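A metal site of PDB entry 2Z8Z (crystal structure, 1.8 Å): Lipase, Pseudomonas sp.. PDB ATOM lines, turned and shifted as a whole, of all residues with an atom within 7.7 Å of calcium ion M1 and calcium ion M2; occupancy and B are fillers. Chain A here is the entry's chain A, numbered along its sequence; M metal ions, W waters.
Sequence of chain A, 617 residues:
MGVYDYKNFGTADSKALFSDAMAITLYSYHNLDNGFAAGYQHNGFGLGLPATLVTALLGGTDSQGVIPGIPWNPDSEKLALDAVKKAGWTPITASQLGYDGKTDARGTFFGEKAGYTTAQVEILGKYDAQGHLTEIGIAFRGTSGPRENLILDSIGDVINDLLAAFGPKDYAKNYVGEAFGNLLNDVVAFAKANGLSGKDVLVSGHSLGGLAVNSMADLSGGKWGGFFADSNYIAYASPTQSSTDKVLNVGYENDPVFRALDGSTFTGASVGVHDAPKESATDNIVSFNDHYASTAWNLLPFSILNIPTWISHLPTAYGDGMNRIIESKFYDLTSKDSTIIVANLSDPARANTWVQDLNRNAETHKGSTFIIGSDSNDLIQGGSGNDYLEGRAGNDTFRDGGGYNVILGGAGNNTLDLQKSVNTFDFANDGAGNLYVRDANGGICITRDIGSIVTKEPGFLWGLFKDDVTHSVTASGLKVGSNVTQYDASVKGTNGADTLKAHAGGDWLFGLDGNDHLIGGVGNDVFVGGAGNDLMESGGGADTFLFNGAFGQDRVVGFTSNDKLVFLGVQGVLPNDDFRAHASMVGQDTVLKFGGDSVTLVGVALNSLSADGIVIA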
ATOM      1  N   ASN A 249     -18.201  21.277  17.960  1.00  0.00           N
ATOM      2  CA  ASN A 249     -18.872  22.111  18.980  1.00  0.00           C
ATOM      3  C   ASN A 249     -18.209  23.476  19.047  1.00  0.00           C
ATOM      4  O   ASN A 249     -17.113  23.639  19.610  1.00  0.00           O
ATOM      5  CB  ASN A 249     -18.848  21.414  20.351  1.00  0.00           C
ATOM      6  CG  ASN A 249     -19.939  20.338  20.484  1.00  0.00           C
ATOM      7  OD1 ASN A 249     -19.640  19.114  20.653  1.00  0.00           O
ATOM      8  ND2 ASN A 249     -21.181  20.744  20.364  1.00  0.00           N
ATOM      9  N   GLU A 253     -16.000  31.246  24.447  1.00  0.00           N
ATOM     10  CA  GLU A 253     -15.401  30.816  25.715  1.00  0.00           C
ATOM     11  C   GLU A 253     -16.189  31.388  26.895  1.00  0.00           C
ATOM     12  O   GLU A 253     -16.300  30.734  27.975  1.00  0.00           O
ATOM     13  CB  GLU A 253     -13.966  31.351  25.759  1.00  0.00           C
ATOM     14  CG  GLU A 253     -13.209  31.109  26.913  1.00  0.00           C
ATOM     15  CD  GLU A 253     -11.812  31.647  26.803  1.00  0.00           C
ATOM     16  OE1 GLU A 253     -11.593  32.864  26.997  1.00  0.00           O
ATOM     17  OE2 GLU A 253     -10.933  30.820  26.629  1.00  0.00           O
ATOM     18  N   ASN A 254     -16.685  32.610  26.717  1.00  0.00           N
ATOM     19  CA  ASN A 254     -17.345  33.341  27.806  1.00  0.00           C
ATOM     20  C   ASN A 254     -18.861  33.171  27.775  1.00  0.00           C
ATOM     21  O   ASN A 254     -19.601  33.845  28.478  1.00  0.00           O
ATOM     22  CB  ASN A 254     -16.898  34.821  27.872  1.00  0.00           C
ATOM     23  CG  ASN A 254     -16.982  35.553  26.573  1.00  0.00           C
ATOM     24  OD1 ASN A 254     -16.666  35.037  25.486  1.00  0.00           O
ATOM     25  ND2 ASN A 254     -17.335  36.847  26.679  1.00  0.00           N
ATOM     26  N   ARG A 259     -20.443  24.282  26.850  1.00  0.00           N
ATOM     27  CA  ARG A 259     -19.600  23.303  27.537  1.00  0.00           C
ATOM     28  C   ARG A 259     -19.933  23.235  29.055  1.00  0.00           C
ATOM     29  O   ARG A 259     -19.095  22.809  29.939  1.00  0.00           O
ATOM     30  CB  ARG A 259     -18.122  23.630  27.336  1.00  0.00           C
ATOM     31  CG  ARG A 259     -17.637  23.736  25.876  1.00  0.00           C
ATOM     32  CD  ARG A 259     -16.194  24.353  25.837  1.00  0.00           C
ATOM     33  NE  ARG A 259     -16.142  25.657  26.478  1.00  0.00           N
ATOM     34  CZ  ARG A 259     -15.034  26.305  26.867  1.00  0.00           C
ATOM     35  NH1 ARG A 259     -13.854  25.737  26.690  1.00  0.00           N
ATOM     36  NH2 ARG A 259     -15.113  27.493  27.451  1.00  0.00           N
ATOM     37  N   HIS A 274     -16.177  26.910  33.261  1.00  0.00           N
ATOM     38  CA  HIS A 274     -16.003  25.548  32.776  1.00  0.00           C
ATOM     39  C   HIS A 274     -15.304  25.581  31.432  1.00  0.00           C
ATOM     40  O   HIS A 274     -15.875  25.270  30.377  1.00  0.00           O
ATOM     41  CB  HIS A 274     -17.356  24.797  32.708  1.00  0.00           C
ATOM     42  CG  HIS A 274     -18.477  25.635  32.221  1.00  0.00           C
ATOM     43  ND1 HIS A 274     -18.633  25.980  30.883  1.00  0.00           N
ATOM     44  CD2 HIS A 274     -19.509  26.221  32.880  1.00  0.00           C
ATOM     45  CE1 HIS A 274     -19.722  26.710  30.758  1.00  0.00           C
ATOM     46  NE2 HIS A 274     -20.268  26.888  31.944  1.00  0.00           N
ATOM     47  N   ASP A 275     -14.004  25.920  31.513  1.00  0.00           N
ATOM     48  CA  ASP A 275     -13.177  26.175  30.374  1.00  0.00           C
ATOM     49  C   ASP A 275     -12.055  25.128  30.165  1.00  0.00           C
ATOM     50  O   ASP A 275     -10.994  25.405  29.511  1.00  0.00           O
ATOM     51  CB  ASP A 275     -12.614  27.561  30.523  1.00  0.00           C
ATOM     52  CG  ASP A 275     -11.953  28.076  29.239  1.00  0.00           C
ATOM     53  OD1 ASP A 275     -12.446  27.804  28.092  1.00  0.00           O
ATOM     54  OD2 ASP A 275     -10.880  28.720  29.401  1.00  0.00           O
ATOM     55  N   ALA A 276     -12.275  23.914  30.693  1.00  0.00           N
ATOM     56  CA  ALA A 276     -11.323  22.849  30.472  1.00  0.00           C
ATOM     57  C   ALA A 276     -11.354  22.443  28.986  1.00  0.00           C
ATOM     58  O   ALA A 276     -12.439  22.475  28.322  1.00  0.00           O
ATOM     59  CB  ALA A 276     -11.558  21.631  31.435  1.00  0.00           C
ATOM     60  N   PRO A 277     -10.171  22.162  28.427  1.00  0.00           N
ATOM     61  CA  PRO A 277     -10.173  21.756  27.040  1.00  0.00           C
ATOM     62  C   PRO A 277     -11.051  20.554  26.712  1.00  0.00           C
ATOM     63  O   PRO A 277     -11.108  19.595  27.460  1.00  0.00           O
ATOM     64  CB  PRO A 277      -8.681  21.461  26.753  1.00  0.00           C
ATOM     65  CG  PRO A 277      -7.978  22.305  27.747  1.00  0.00           C
ATOM     66  CD  PRO A 277      -8.792  22.266  28.966  1.00  0.00           C
ATOM     67  N   LYS A 278     -11.689  20.608  25.531  1.00  0.00           N
ATOM     68  CA  LYS A 278     -12.487  19.498  25.048  1.00  0.00           C
ATOM     69  C   LYS A 278     -12.196  19.207  23.616  1.00  0.00           C
ATOM     70  O   LYS A 278     -12.152  20.130  22.793  1.00  0.00           O
ATOM     71  CB  LYS A 278     -13.960  19.835  25.240  1.00  0.00           C
ATOM     72  CG  LYS A 278     -14.397  19.711  26.753  1.00  0.00           C
ATOM     73  CD  LYS A 278     -15.846  20.189  27.030  1.00  0.00           C
ATOM     74  CE  LYS A 278     -16.307  19.749  28.501  1.00  0.00           C
ATOM     75  NZ  LYS A 278     -15.414  20.349  29.509  1.00  0.00           N
ATOM     76  N   GLU A 279     -11.966  17.937  23.299  1.00  0.00           N
ATOM     77  CA  GLU A 279     -11.557  17.552  21.950  1.00  0.00           C
ATOM     78  C   GLU A 279     -12.501  17.991  20.824  1.00  0.00           C
ATOM     79  O   GLU A 279     -12.070  18.407  19.745  1.00  0.00           O
ATOM     80  CB  GLU A 279     -11.341  16.042  21.872  1.00  0.00           C
ATOM     81  CG  GLU A 279     -10.737  15.570  20.553  1.00  0.00           C
ATOM     82  CD  GLU A 279     -11.773  15.286  19.471  1.00  0.00           C
ATOM     83  OE1 GLU A 279     -13.001  15.155  19.802  1.00  0.00           O
ATOM     84  OE2 GLU A 279     -11.350  15.166  18.263  1.00  0.00           O
ATOM     85  N   SER A 280     -13.797  17.871  21.032  1.00  0.00           N
ATOM     86  CA  SER A 280     -14.748  18.281  20.040  1.00  0.00           C
ATOM     87  C   SER A 280     -14.980  19.825  19.864  1.00  0.00           C
ATOM     88  O   SER A 280     -15.600  20.282  18.888  1.00  0.00           O
ATOM     89  CB  SER A 280     -16.097  17.633  20.348  1.00  0.00           C
ATOM     90  OG  SER A 280     -16.785  18.332  21.377  1.00  0.00           O
ATOM     91  N   ALA A 281     -14.514  20.626  20.831  1.00  0.00           N
ATOM     92  CA  ALA A 281     -14.890  22.045  20.927  1.00  0.00           C
ATOM     93  C   ALA A 281     -13.798  23.026  20.570  1.00  0.00           C
ATOM     94  O   ALA A 281     -12.624  22.779  20.820  1.00  0.00           O
ATOM     95  CB  ALA A 281     -15.315  22.318  22.321  1.00  0.00           C
ATOM     96  N   THR A 282     -14.195  24.206  20.071  1.00  0.00           N
ATOM     97  CA  THR A 282     -13.325  25.351  19.957  1.00  0.00           C
ATOM     98  C   THR A 282     -13.248  26.015  21.347  1.00  0.00           C
ATOM     99  O   THR A 282     -14.211  26.527  21.831  1.00  0.00           O
ATOM    100  CB  THR A 282     -13.871  26.367  18.954  1.00  0.00           C
ATOM    101  OG1 THR A 282     -15.178  26.710  19.368  1.00  0.00           O
ATOM    102  CG2 THR A 282     -13.938  25.753  17.554  1.00  0.00           C
ATOM    103  N   ASP A 283     -12.109  25.940  21.993  1.00  0.00           N
ATOM    104  CA  ASP A 283     -12.047  26.309  23.397  1.00  0.00           C
ATOM    105  C   ASP A 283     -11.665  27.752  23.761  1.00  0.00           C
ATOM    106  O   ASP A 283     -11.780  28.100  24.937  1.00  0.00           O
ATOM    107  CB  ASP A 283     -11.179  25.315  24.165  1.00  0.00           C
ATOM    108  CG  ASP A 283     -11.827  23.918  24.261  1.00  0.00           C
ATOM    109  OD1 ASP A 283     -13.009  23.839  24.694  1.00  0.00           O
ATOM    110  OD2 ASP A 283     -11.162  22.896  23.930  1.00  0.00           O
ATOM    111  N   ASN A 284     -11.255  28.575  22.791  1.00  0.00           N
ATOM    112  CA  ASN A 284     -10.593  29.830  23.108  1.00  0.00           C
ATOM    113  C   ASN A 284     -11.022  30.989  22.211  1.00  0.00           C
ATOM    114  O   ASN A 284     -10.225  31.841  21.938  1.00  0.00           O
ATOM    115  CB  ASN A 284      -9.052  29.657  23.052  1.00  0.00           C
ATOM    116  CG  ASN A 284      -8.565  28.526  23.910  1.00  0.00           C
ATOM    117  OD1 ASN A 284      -7.928  27.560  23.441  1.00  0.00           O
ATOM    118  ND2 ASN A 284      -8.816  28.657  25.204  1.00  0.00           N
ATOM    119  N   ILE A 285     -12.286  31.011  21.851  1.00  0.00           N
ATOM    120  CA  ILE A 285     -12.842  32.127  21.075  1.00  0.00           C
ATOM    121  C   ILE A 285     -13.596  33.031  22.041  1.00  0.00           C
ATOM    122  O   ILE A 285     -14.653  32.652  22.570  1.00  0.00           O
ATOM    123  CB  ILE A 285     -13.810  31.653  19.962  1.00  0.00           C
ATOM    124  CG1 ILE A 285     -13.166  30.599  19.009  1.00  0.00           C
ATOM    125  CG2 ILE A 285     -14.206  32.858  19.086  1.00  0.00           C
ATOM    126  CD1 ILE A 285     -14.080  29.996  18.014  1.00  0.00           C
ATOM    127  N   VAL A 286     -13.111  34.266  22.187  1.00  0.00           N
ATOM    128  CA  VAL A 286     -13.695  35.222  23.147  1.00  0.00           C
ATOM    129  C   VAL A 286     -14.641  36.143  22.488  1.00  0.00           C
ATOM    130  O   VAL A 286     -14.318  36.702  21.432  1.00  0.00           O
ATOM    131  CB  VAL A 286     -12.611  36.053  23.832  1.00  0.00           C
ATOM    132  CG1 VAL A 286     -13.194  37.155  24.699  1.00  0.00           C
ATOM    133  CG2 VAL A 286     -11.725  35.197  24.614  1.00  0.00           C
ATOM    134  N   LYS A 336      -8.312  24.779  15.784  1.00  0.00           N
ATOM    135  CA  LYS A 336      -9.566  24.639  16.526  1.00  0.00           C
ATOM    136  C   LYS A 336      -9.503  25.359  17.869  1.00  0.00           C
ATOM    137  O   LYS A 336     -10.485  25.950  18.294  1.00  0.00           O
ATOM    138  CB  LYS A 336      -9.845  23.156  16.756  1.00  0.00           C
ATOM    139  CG  LYS A 336     -11.224  22.842  17.294  1.00  0.00           C
ATOM    140  CD  LYS A 336     -11.496  21.393  17.061  1.00  0.00           C
ATOM    141  CE  LYS A 336     -12.825  20.903  17.566  1.00  0.00           C
ATOM    142  NZ  LYS A 336     -13.038  19.545  16.894  1.00  0.00           N
ATOM    143  N   ASP A 337      -8.336  25.316  18.516  1.00  0.00           N
ATOM    144  CA  ASP A 337      -8.150  25.921  19.837  1.00  0.00           C
ATOM    145  C   ASP A 337      -7.264  27.180  19.852  1.00  0.00           C
ATOM    146  O   ASP A 337      -6.797  27.619  20.898  1.00  0.00           O
ATOM    147  CB  ASP A 337      -7.673  24.861  20.872  1.00  0.00           C
ATOM    148  CG  ASP A 337      -8.727  23.842  21.169  1.00  0.00           C
ATOM    149  OD1 ASP A 337      -9.923  24.236  21.264  1.00  0.00           O
ATOM    150  OD2 ASP A 337      -8.374  22.663  21.297  1.00  0.00           O
ATOM    151  N   SER A 338      -7.121  27.821  18.692  1.00  0.00           N
ATOM    152  CA  SER A 338      -6.522  29.152  18.646  1.00  0.00           C
ATOM    153  C   SER A 338      -7.303  30.109  19.507  1.00  0.00           C
ATOM    154  O   SER A 338      -8.525  30.047  19.645  1.00  0.00           O
ATOM    155  CB  SER A 338      -6.457  29.693  17.191  1.00  0.00           C
ATOM    156  OG  SER A 338      -5.592  28.956  16.347  1.00  0.00           O
ATOM    157  N   THR A 339      -6.570  30.977  20.166  1.00  0.00           N
ATOM    158  CA  THR A 339      -7.109  32.110  20.896  1.00  0.00           C
ATOM    159  C   THR A 339      -7.511  33.189  19.873  1.00  0.00           C
ATOM    160  O   THR A 339      -6.684  33.770  19.140  1.00  0.00           O
ATOM    161  CB  THR A 339      -6.093  32.746  21.804  1.00  0.00           C
ATOM    162  OG1 THR A 339      -5.421  31.749  22.596  1.00  0.00           O
ATOM    163  CG2 THR A 339      -6.773  33.827  22.696  1.00  0.00           C
ATOM    164  N   ASN A 359      -8.143  37.623  29.152  1.00  0.00           N
ATOM    165  CA  ASN A 359      -8.114  36.251  29.699  1.00  0.00           C
ATOM    166  C   ASN A 359      -9.049  36.084  30.899  1.00  0.00           C
ATOM    167  O   ASN A 359      -8.761  35.348  31.825  1.00  0.00           O
ATOM    168  CB  ASN A 359      -6.699  35.853  30.111  1.00  0.00           C
ATOM    169  CG  ASN A 359      -6.375  34.378  29.785  1.00  0.00           C
ATOM    170  OD1 ASN A 359      -5.365  34.121  29.124  1.00  0.00           O
ATOM    171  ND2 ASN A 359      -7.243  33.430  30.210  1.00  0.00           N
ATOM    172  N   ASN A 361     -12.031  34.845  33.196  1.00  0.00           N
ATOM    173  CA  ASN A 361     -12.939  33.705  33.329  1.00  0.00           C
ATOM    174  C   ASN A 361     -12.613  32.583  32.358  1.00  0.00           C
ATOM    175  O   ASN A 361     -13.476  32.065  31.643  1.00  0.00           O
ATOM    176  CB  ASN A 361     -14.375  34.191  33.162  1.00  0.00           C
ATOM    177  CG  ASN A 361     -14.828  35.026  34.303  1.00  0.00           C
ATOM    178  OD1 ASN A 361     -14.515  34.724  35.472  1.00  0.00           O
ATOM    179  ND2 ASN A 361     -15.582  36.057  33.998  1.00  0.00           N
ATOM    180  N   ALA A 362     -11.350  32.209  32.345  1.00  0.00           N
ATOM    181  CA  ALA A 362     -10.806  31.269  31.353  1.00  0.00           C
ATOM    182  C   ALA A 362      -9.466  30.757  31.816  1.00  0.00           C
ATOM    183  O   ALA A 362      -8.709  31.470  32.525  1.00  0.00           O
ATOM    184  CB  ALA A 362     -10.664  32.003  29.958  1.00  0.00           C
ATOM    185  N   GLU A 363      -9.118  29.546  31.389  1.00  0.00           N
ATOM    186  CA  GLU A 363      -7.789  29.022  31.606  1.00  0.00           C
ATOM    187  C   GLU A 363      -6.800  29.891  30.847  1.00  0.00           C
ATOM    188  O   GLU A 363      -7.183  30.566  29.913  1.00  0.00           O
ATOM    189  CB  GLU A 363      -7.759  27.589  31.125  1.00  0.00           C
ATOM    190  CG  GLU A 363      -8.786  26.759  31.944  1.00  0.00           C
ATOM    191  CD  GLU A 363      -8.567  25.294  32.050  1.00  0.00           C
ATOM    192  OE1 GLU A 363      -7.701  24.765  31.352  1.00  0.00           O
ATOM    193  OE2 GLU A 363      -9.384  24.673  32.829  1.00  0.00           O
ATOM    194  N   THR A 364      -5.536  29.872  31.232  1.00  0.00           N
ATOM    195  CA  THR A 364      -4.522  30.670  30.592  1.00  0.00           C
ATOM    196  C   THR A 364      -4.365  30.360  29.122  1.00  0.00           C
ATOM    197  O   THR A 364      -4.251  29.239  28.741  1.00  0.00           O
ATOM    198  CB  THR A 364      -3.175  30.547  31.310  1.00  0.00           C
ATOM    199  OG1 THR A 364      -3.381  31.057  32.643  1.00  0.00           O
ATOM    200  CG2 THR A 364      -2.115  31.363  30.616  1.00  0.00           C
ATOM    201  N   HIS A 365      -4.433  31.383  28.310  1.00  0.00           N
ATOM    202  CA  HIS A 365      -4.380  31.173  26.897  1.00  0.00           C
ATOM    203  C   HIS A 365      -2.984  30.851  26.470  1.00  0.00           C
ATOM    204  O   HIS A 365      -2.045  31.416  27.019  1.00  0.00           O
ATOM    205  CB  HIS A 365      -4.840  32.401  26.156  1.00  0.00           C
ATOM    206  CG  HIS A 365      -6.334  32.643  26.243  1.00  0.00           C
ATOM    207  ND1 HIS A 365      -6.840  33.910  26.331  1.00  0.00           N
ATOM    208  CD2 HIS A 365      -7.385  31.792  26.334  1.00  0.00           C
ATOM    209  CE1 HIS A 365      -8.176  33.837  26.411  1.00  0.00           C
ATOM    210  NE2 HIS A 365      -8.530  32.576  26.381  1.00  0.00           N
HETATM  211 CA    CA M   1     -10.439  28.619  26.930  1.00  0.00          CA
HETATM  212 CA    CA M   2     -10.652  21.918  21.915  1.00  0.00          CA
HETATM  213  O   HOH W   1      -9.114  20.535  23.197  1.00  0.00           O
HETATM  214  O   HOH W   2      -9.859  26.249  27.301  1.00  0.00           O
HETATM  215  O   HOH W   3      -8.272  29.165  27.776  1.00  0.00           O
HETATM  216  O   HOH W   4     -10.263  20.510  20.118  1.00  0.00           O
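The nearest printed residue that does not touch calcium ion M2 is Glu 279 (4.4 Å).
OD1 of Asp 283 lies within salt-bridge range of NH1 of Arg 259, 2.9 Å away. The side-chain carboxylate (OD2) of Asp 275 lies close to the backbone NH (N) of Glu 363 (2.8 Å). O of Glu 253 is in hydrogen-bond range of NH2 of Arg 259, 3.5 Å away. N of Glu 253 lies within hydrogen-bond range of O of Ile 285, 2.7 Å away. OD1 of Asp 275 lies close to NH2 of Arg 259, 2.8 Å away. The side-chain carboxylate of Glu 253 sits at hydrogen-bond distance from a ring nitrogen (NE2) of His 365, at 3.1 Å. The backbone carbonyl oxygen (O) of Asp 337 sits close to the side-chain amide oxygen (OD1) of Asn 284, at 2.8 Å.
Calcium ion M2 is bound by OD2 of Asp 283 (2.3 Å), water W4 (2.3 Å), O of Ala 281 (2.4 Å), water W1 (2.4 Å), OD2 of Asp 337 (2.5 Å), O of Lys 278 (2.5 Å) and OD1 of Asp 337 (2.5 Å).
Calcium ion M1 is bound by the side-chain carboxylate (OE2) of Glu 253 (2.3 Å), the side-chain amide nitrogen (ND2) of Asn 284 (2.4 Å), water W3 (2.4 Å), the backbone carbonyl oxygen (O) of Asp 283 (2.5 Å), the side-chain carboxylate (OD1) of Asp 275 (2.5 Å), water W2 (2.5 Å) and the side-chain carboxylate (OD2) of Asp 275 (2.5 Å). Calcium ion M1 has seven donor atoms within binding distance.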
